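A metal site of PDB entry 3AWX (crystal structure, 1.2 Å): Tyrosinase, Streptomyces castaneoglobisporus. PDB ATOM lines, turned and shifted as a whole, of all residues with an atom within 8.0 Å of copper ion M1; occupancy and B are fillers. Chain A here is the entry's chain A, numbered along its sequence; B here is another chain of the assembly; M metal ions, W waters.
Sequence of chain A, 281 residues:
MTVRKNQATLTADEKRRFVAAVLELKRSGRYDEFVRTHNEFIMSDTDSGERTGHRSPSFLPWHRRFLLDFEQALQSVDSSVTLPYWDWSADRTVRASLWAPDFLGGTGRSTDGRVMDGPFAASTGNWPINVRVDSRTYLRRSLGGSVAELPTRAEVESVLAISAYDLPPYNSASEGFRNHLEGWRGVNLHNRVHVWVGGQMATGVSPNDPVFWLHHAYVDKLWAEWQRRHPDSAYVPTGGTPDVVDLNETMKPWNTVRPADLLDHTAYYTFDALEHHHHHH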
ATOM      1  N   HIS A  38       0.310  23.430  17.145  1.00  0.00           N
ATOM      2  CA  HIS A  38      -0.581  23.860  18.227  1.00  0.00           C
ATOM      3  C   HIS A  38      -1.781  22.944  18.397  1.00  0.00           C
ATOM      4  O   HIS A  38      -2.154  22.552  19.506  1.00  0.00           O
ATOM      5  CB  HIS A  38      -1.061  25.299  17.939  1.00  0.00           C
ATOM      6  CG  HIS A  38      -1.876  25.801  19.121  1.00  0.00           C
ATOM      7  ND1 HIS A  38      -3.260  25.746  19.141  1.00  0.00           N
ATOM      8  CD2 HIS A  38      -1.524  26.345  20.323  1.00  0.00           C
ATOM      9  CE1 HIS A  38      -3.689  26.249  20.306  1.00  0.00           C
ATOM     10  NE2 HIS A  38      -2.650  26.638  21.052  1.00  0.00           N
ATOM     11  N   ILE A  42      -2.972  20.890  21.716  1.00  0.00           N
ATOM     12  CA  ILE A  42      -4.182  21.230  22.467  1.00  0.00           C
ATOM     13  C   ILE A  42      -5.135  20.057  22.462  1.00  0.00           C
ATOM     14  O   ILE A  42      -5.941  19.861  23.383  1.00  0.00           O
ATOM     15  CB  ILE A  42      -4.806  22.528  21.915  1.00  0.00           C
ATOM     16  CG1 ILE A  42      -5.716  23.163  22.987  1.00  0.00           C
ATOM     17  CG2 ILE A  42      -5.478  22.313  20.591  1.00  0.00           C
ATOM     18  CD1 ILE A  42      -6.317  24.484  22.537  1.00  0.00           C
ATOM     19  N   GLY A  53       1.145  21.801  26.794  1.00  0.00           N
ATOM     20  CA  GLY A  53       0.956  23.140  26.246  1.00  0.00           C
ATOM     21  C   GLY A  53      -0.136  23.952  26.910  1.00  0.00           C
ATOM     22  O   GLY A  53      -0.166  25.175  26.856  1.00  0.00           O
ATOM     23  N   HIS A  54      -1.110  23.272  27.507  1.00  0.00           N
ATOM     24  CA  HIS A  54      -2.340  23.826  28.014  1.00  0.00           C
ATOM     25  C   HIS A  54      -2.701  23.155  29.335  1.00  0.00           C
ATOM     26  O   HIS A  54      -2.247  22.065  29.664  1.00  0.00           O
ATOM     27  CB  HIS A  54      -3.508  23.587  26.998  1.00  0.00           C
ATOM     28  CG  HIS A  54      -3.153  24.203  25.654  1.00  0.00           C
ATOM     29  ND1 HIS A  54      -2.421  23.555  24.693  1.00  0.00           N
ATOM     30  CD2 HIS A  54      -3.421  25.462  25.171  1.00  0.00           C
ATOM     31  CE1 HIS A  54      -2.244  24.427  23.682  1.00  0.00           C
ATOM     32  NE2 HIS A  54      -2.864  25.598  23.939  1.00  0.00           N
ATOM     33  N   PHE A  59       1.786  25.737  30.463  1.00  0.00           N
ATOM     34  CA  PHE A  59       1.062  26.568  29.500  1.00  0.00           C
ATOM     35  C   PHE A  59       1.861  27.845  29.159  1.00  0.00           C
ATOM     36  O   PHE A  59       1.985  28.204  27.961  1.00  0.00           O
ATOM     37  CB  PHE A  59      -0.265  26.960  30.118  1.00  0.00           C
ATOM     38  CG  PHE A  59      -1.041  28.112  29.410  1.00  0.00           C
ATOM     39  CD1 PHE A  59      -1.582  27.939  28.148  1.00  0.00           C
ATOM     40  CD2 PHE A  59      -1.209  29.310  30.087  1.00  0.00           C
ATOM     41  CE1 PHE A  59      -2.271  28.974  27.534  1.00  0.00           C
ATOM     42  CE2 PHE A  59      -1.918  30.356  29.452  1.00  0.00           C
ATOM     43  CZ  PHE A  59      -2.460  30.171  28.203  1.00  0.00           C
ATOM     44  N   HIS A  63       3.898  28.278  25.532  1.00  0.00           N
ATOM     45  CA  HIS A  63       3.535  29.295  24.532  1.00  0.00           C
ATOM     46  C   HIS A  63       4.643  30.321  24.367  1.00  0.00           C
ATOM     47  O   HIS A  63       4.819  30.881  23.285  1.00  0.00           O
ATOM     48  CB  HIS A  63       2.199  29.965  24.906  1.00  0.00           C
ATOM     49  CG  HIS A  63       1.025  29.073  24.587  1.00  0.00           C
ATOM     50  ND1 HIS A  63       0.605  28.049  25.442  1.00  0.00           N
ATOM     51  CD2 HIS A  63       0.233  28.998  23.480  1.00  0.00           C
ATOM     52  CE1 HIS A  63      -0.409  27.396  24.899  1.00  0.00           C
ATOM     53  NE2 HIS A  63      -0.676  27.964  23.712  1.00  0.00           N
ATOM     54  N   GLU A 182      -4.850  31.634  32.306  1.00  0.00           N
ATOM     55  CA  GLU A 182      -5.323  30.759  31.200  1.00  0.00           C
ATOM     56  C   GLU A 182      -6.821  30.891  31.035  1.00  0.00           C
ATOM     57  O   GLU A 182      -7.322  31.065  29.926  1.00  0.00           O
ATOM     58  CB  GLU A 182      -4.852  29.324  31.461  1.00  0.00           C
ATOM     59  CG  GLU A 182      -5.099  28.433  30.237  1.00  0.00           C
ATOM     60  CD  GLU A 182      -4.551  27.045  30.375  1.00  0.00           C
ATOM     61  OE1 GLU A 182      -3.872  26.758  31.381  1.00  0.00           O
ATOM     62  OE2 GLU A 182      -4.808  26.245  29.444  1.00  0.00           O
ATOM     63  N   HIS A 190      -7.391  34.552  29.253  1.00  0.00           N
ATOM     64  CA  HIS A 190      -6.937  34.125  27.927  1.00  0.00           C
ATOM     65  C   HIS A 190      -7.967  33.328  27.159  1.00  0.00           C
ATOM     66  O   HIS A 190      -8.121  33.534  25.946  1.00  0.00           O
ATOM     67  CB  HIS A 190      -5.644  33.258  28.130  1.00  0.00           C
ATOM     68  CG  HIS A 190      -5.447  32.177  27.109  1.00  0.00           C
ATOM     69  ND1 HIS A 190      -6.035  30.938  27.249  1.00  0.00           N
ATOM     70  CD2 HIS A 190      -4.769  32.131  25.955  1.00  0.00           C
ATOM     71  CE1 HIS A 190      -5.706  30.183  26.202  1.00  0.00           C
ATOM     72  NE2 HIS A 190      -4.922  30.887  25.364  1.00  0.00           N
ATOM     73  N   ASN A 191      -8.715  32.429  27.838  1.00  0.00           N
ATOM     74  CA  ASN A 191      -9.701  31.630  27.055  1.00  0.00           C
ATOM     75  C   ASN A 191     -10.795  32.516  26.507  1.00  0.00           C
ATOM     76  O   ASN A 191     -11.218  32.369  25.360  1.00  0.00           O
ATOM     77  CB  ASN A 191     -10.332  30.541  27.910  1.00  0.00           C
ATOM     78  CG  ASN A 191      -9.429  29.368  28.199  1.00  0.00           C
ATOM     79  OD1 ASN A 191      -8.321  29.227  27.670  1.00  0.00           O
ATOM     80  ND2 ASN A 191      -9.904  28.514  29.103  1.00  0.00           N
ATOM     81  N   VAL A 193     -10.675  35.616  25.558  1.00  0.00           N
ATOM     82  CA  VAL A 193     -10.291  36.345  24.353  1.00  0.00           C
ATOM     83  C   VAL A 193     -10.407  35.460  23.101  1.00  0.00           C
ATOM     84  O   VAL A 193     -10.894  35.926  22.061  1.00  0.00           O
ATOM     85  CB  VAL A 193      -8.869  36.899  24.505  1.00  0.00           C
ATOM     86  CG1 VAL A 193      -8.415  37.552  23.180  1.00  0.00           C
ATOM     87  CG2 VAL A 193      -8.780  37.878  25.692  1.00  0.00           C
ATOM     88  N   HIS A 194      -9.987  34.167  23.200  1.00  0.00           N
ATOM     89  CA  HIS A 194     -10.216  33.290  22.056  1.00  0.00           C
ATOM     90  C   HIS A 194     -11.689  33.221  21.673  1.00  0.00           C
ATOM     91  O   HIS A 194     -12.038  33.273  20.476  1.00  0.00           O
ATOM     92  CB  HIS A 194      -9.696  31.909  22.379  1.00  0.00           C
ATOM     93  CG  HIS A 194      -8.237  31.634  22.289  1.00  0.00           C
ATOM     94  ND1 HIS A 194      -7.605  31.338  21.077  1.00  0.00           N
ATOM     95  CD2 HIS A 194      -7.256  31.530  23.225  1.00  0.00           C
ATOM     96  CE1 HIS A 194      -6.309  31.079  21.326  1.00  0.00           C
ATOM     97  NE2 HIS A 194      -6.067  31.193  22.619  1.00  0.00           N
ATOM     98  N   MET A 201     -10.022  31.262  15.601  1.00  0.00           N
ATOM     99  CA  MET A 201      -9.383  31.599  16.874  1.00  0.00           C
ATOM    100  C   MET A 201     -10.037  30.942  18.047  1.00  0.00           C
ATOM    101  O   MET A 201      -9.455  30.848  19.135  1.00  0.00           O
ATOM    102  CB  MET A 201      -9.404  33.117  16.951  1.00  0.00           C
ATOM    103  CG  MET A 201      -8.643  33.716  18.100  1.00  0.00           C
ATOM    104  SD  MET A 201      -6.868  33.356  18.162  1.00  0.00           S
ATOM    105  CE  MET A 201      -6.603  34.378  19.614  1.00  0.00           C
ATOM    106  N   THR A 203     -10.986  27.767  18.060  1.00  0.00           N
ATOM    107  CA  THR A 203     -10.787  26.330  17.845  1.00  0.00           C
ATOM    108  C   THR A 203      -9.355  25.892  18.123  1.00  0.00           C
ATOM    109  O   THR A 203      -8.474  26.696  18.382  1.00  0.00           O
ATOM    110  CB  THR A 203     -11.138  25.908  16.407  1.00  0.00           C
ATOM    111  OG1 THR A 203     -10.075  26.338  15.509  1.00  0.00           O
ATOM    112  CG2 THR A 203     -12.443  26.583  15.992  1.00  0.00           C
ATOM    113  N   SER A 206      -6.462  27.558  16.224  1.00  0.00           N
ATOM    114  CA  SER A 206      -6.498  28.994  16.413  1.00  0.00           C
ATOM    115  C   SER A 206      -5.299  29.754  15.830  1.00  0.00           C
ATOM    116  O   SER A 206      -5.548  30.935  15.471  1.00  0.00           O
ATOM    117  CB  SER A 206      -6.688  29.263  17.910  1.00  0.00           C
ATOM    118  OG  SER A 206      -5.683  28.592  18.670  1.00  0.00           O
ATOM    119  N   PRO A 207      -4.096  29.221  15.669  1.00  0.00           N
ATOM    120  CA  PRO A 207      -3.064  30.016  14.959  1.00  0.00           C
ATOM    121  C   PRO A 207      -3.386  30.290  13.512  1.00  0.00           C
ATOM    122  O   PRO A 207      -2.652  31.060  12.891  1.00  0.00           O
ATOM    123  CB  PRO A 207      -1.764  29.180  15.136  1.00  0.00           C
ATOM    124  CG  PRO A 207      -2.055  28.341  16.359  1.00  0.00           C
ATOM    125  CD  PRO A 207      -3.491  27.979  16.222  1.00  0.00           C
ATOM    126  N   PHE A 212      -3.718  35.332  16.760  1.00  0.00           N
ATOM    127  CA  PHE A 212      -3.267  34.369  17.770  1.00  0.00           C
ATOM    128  C   PHE A 212      -1.970  34.830  18.433  1.00  0.00           C
ATOM    129  O   PHE A 212      -1.796  34.750  19.647  1.00  0.00           O
ATOM    130  CB  PHE A 212      -3.078  33.010  17.096  1.00  0.00           C
ATOM    131  CG  PHE A 212      -2.459  31.927  17.990  1.00  0.00           C
ATOM    132  CD1 PHE A 212      -1.088  31.787  18.174  1.00  0.00           C
ATOM    133  CD2 PHE A 212      -3.329  31.063  18.625  1.00  0.00           C
ATOM    134  CE1 PHE A 212      -0.562  30.836  19.002  1.00  0.00           C
ATOM    135  CE2 PHE A 212      -2.791  30.070  19.433  1.00  0.00           C
ATOM    136  CZ  PHE A 212      -1.422  29.954  19.645  1.00  0.00           C
ATOM    137  N   HIS A 215      -2.376  37.979  20.669  1.00  0.00           N
ATOM    138  CA  HIS A 215      -3.033  37.589  21.921  1.00  0.00           C
ATOM    139  C   HIS A 215      -2.000  36.938  22.819  1.00  0.00           C
ATOM    140  O   HIS A 215      -1.787  37.319  23.995  1.00  0.00           O
ATOM    141  CB  HIS A 215      -4.174  36.632  21.587  1.00  0.00           C
ATOM    142  CG  HIS A 215      -4.833  36.071  22.802  1.00  0.00           C
ATOM    143  ND1 HIS A 215      -4.948  36.820  23.964  1.00  0.00           N
ATOM    144  CD2 HIS A 215      -5.392  34.839  23.017  1.00  0.00           C
ATOM    145  CE1 HIS A 215      -5.602  36.044  24.837  1.00  0.00           C
ATOM    146  NE2 HIS A 215      -5.887  34.841  24.328  1.00  0.00           N
ATOM    147  N   HIS A 216      -1.344  35.881  22.297  1.00  0.00           N
ATOM    148  CA  HIS A 216      -0.380  35.189  23.188  1.00  0.00           C
ATOM    149  C   HIS A 216       0.810  36.050  23.541  1.00  0.00           C
ATOM    150  O   HIS A 216       1.408  35.832  24.610  1.00  0.00           O
ATOM    151  CB  HIS A 216       0.039  33.839  22.566  1.00  0.00           C
ATOM    152  CG  HIS A 216      -0.951  32.786  23.034  1.00  0.00           C
ATOM    153  ND1 HIS A 216      -0.763  32.228  24.288  1.00  0.00           N
ATOM    154  CD2 HIS A 216      -2.081  32.245  22.520  1.00  0.00           C
ATOM    155  CE1 HIS A 216      -1.771  31.366  24.508  1.00  0.00           C
ATOM    156  NE2 HIS A 216      -2.583  31.349  23.456  1.00  0.00           N
ATOM    157  N   VAL A 219      -0.560  37.758  26.630  1.00  0.00           N
ATOM    158  CA  VAL A 219      -0.574  36.784  27.728  1.00  0.00           C
ATOM    159  C   VAL A 219       0.827  36.609  28.304  1.00  0.00           C
ATOM    160  O   VAL A 219       1.012  36.558  29.505  1.00  0.00           O
ATOM    161  CB  VAL A 219      -1.167  35.445  27.231  1.00  0.00           C
ATOM    162  CG1 VAL A 219      -0.990  34.339  28.279  1.00  0.00           C
ATOM    163  CG2 VAL A 219      -2.649  35.612  26.878  1.00  0.00           C
ATOM    164  N   TYR B  98     -11.942  26.481  23.865  1.00  0.00           N
ATOM    165  CA  TYR B  98     -11.640  27.408  24.971  1.00  0.00           C
ATOM    166  C   TYR B  98     -12.917  27.775  25.733  1.00  0.00           C
ATOM    167  O   TYR B  98     -12.951  28.749  26.491  1.00  0.00           O
ATOM    168  CB  TYR B  98     -10.985  28.684  24.443  1.00  0.00           C
ATOM    169  CG  TYR B  98      -9.716  28.435  23.606  1.00  0.00           C
ATOM    170  CD1 TYR B  98      -9.797  28.367  22.221  1.00  0.00           C
ATOM    171  CD2 TYR B  98      -8.474  28.270  24.185  1.00  0.00           C
ATOM    172  CE1 TYR B  98      -8.672  28.143  21.422  1.00  0.00           C
ATOM    173  CE2 TYR B  98      -7.318  28.052  23.429  1.00  0.00           C
ATOM    174  CZ  TYR B  98      -7.436  27.983  22.041  1.00  0.00           C
ATOM    175  OH  TYR B  98      -6.317  27.819  21.270  1.00  0.00           O
HETATM  176 CU    CU M   1      -4.447  30.314  23.542  1.00  0.00          CU
HETATM  177 CU    CU M   2      -3.093  27.367  22.981  1.00  0.00          CU
HETATM  178  O   HOH W   1      -4.117  28.911  22.230  1.00  0.00           O
HETATM  179  O   HOH W   2      -3.807  28.414  24.414  1.00  0.00           O
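O of His 190 lies within hydrogen-bond range of NE2 of His 215, 3.1 Å away.
The side-chain amide oxygen (OD1) of Asn 191 lies within hydrogen-bond range of a ring nitrogen (ND1) of His 190.
ND1 of His 190 is in hydrogen-bond range of O of Glu 182, at 3.0 Å.
ND1 of His 194 sits at hydrogen-bond distance from O of Met 201 (2.7 Å).
The side-chain hydroxyl (OG) of Ser 206 sits at hydrogen-bond distance from the side-chain hydroxyl (OH) of Tyr 98 of chain B.
CE2 of Tyr 98 of chain B touches copper ion M1 (3.7 Å).
Within 4 Å of copper ion M1: His 190, His 194, His 216 and Tyr 98 of chain B.
Copper ion M1 is bound by water W1, NE2 of His 190, NE2 of His 194, NE2 of His 216 and water W2.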
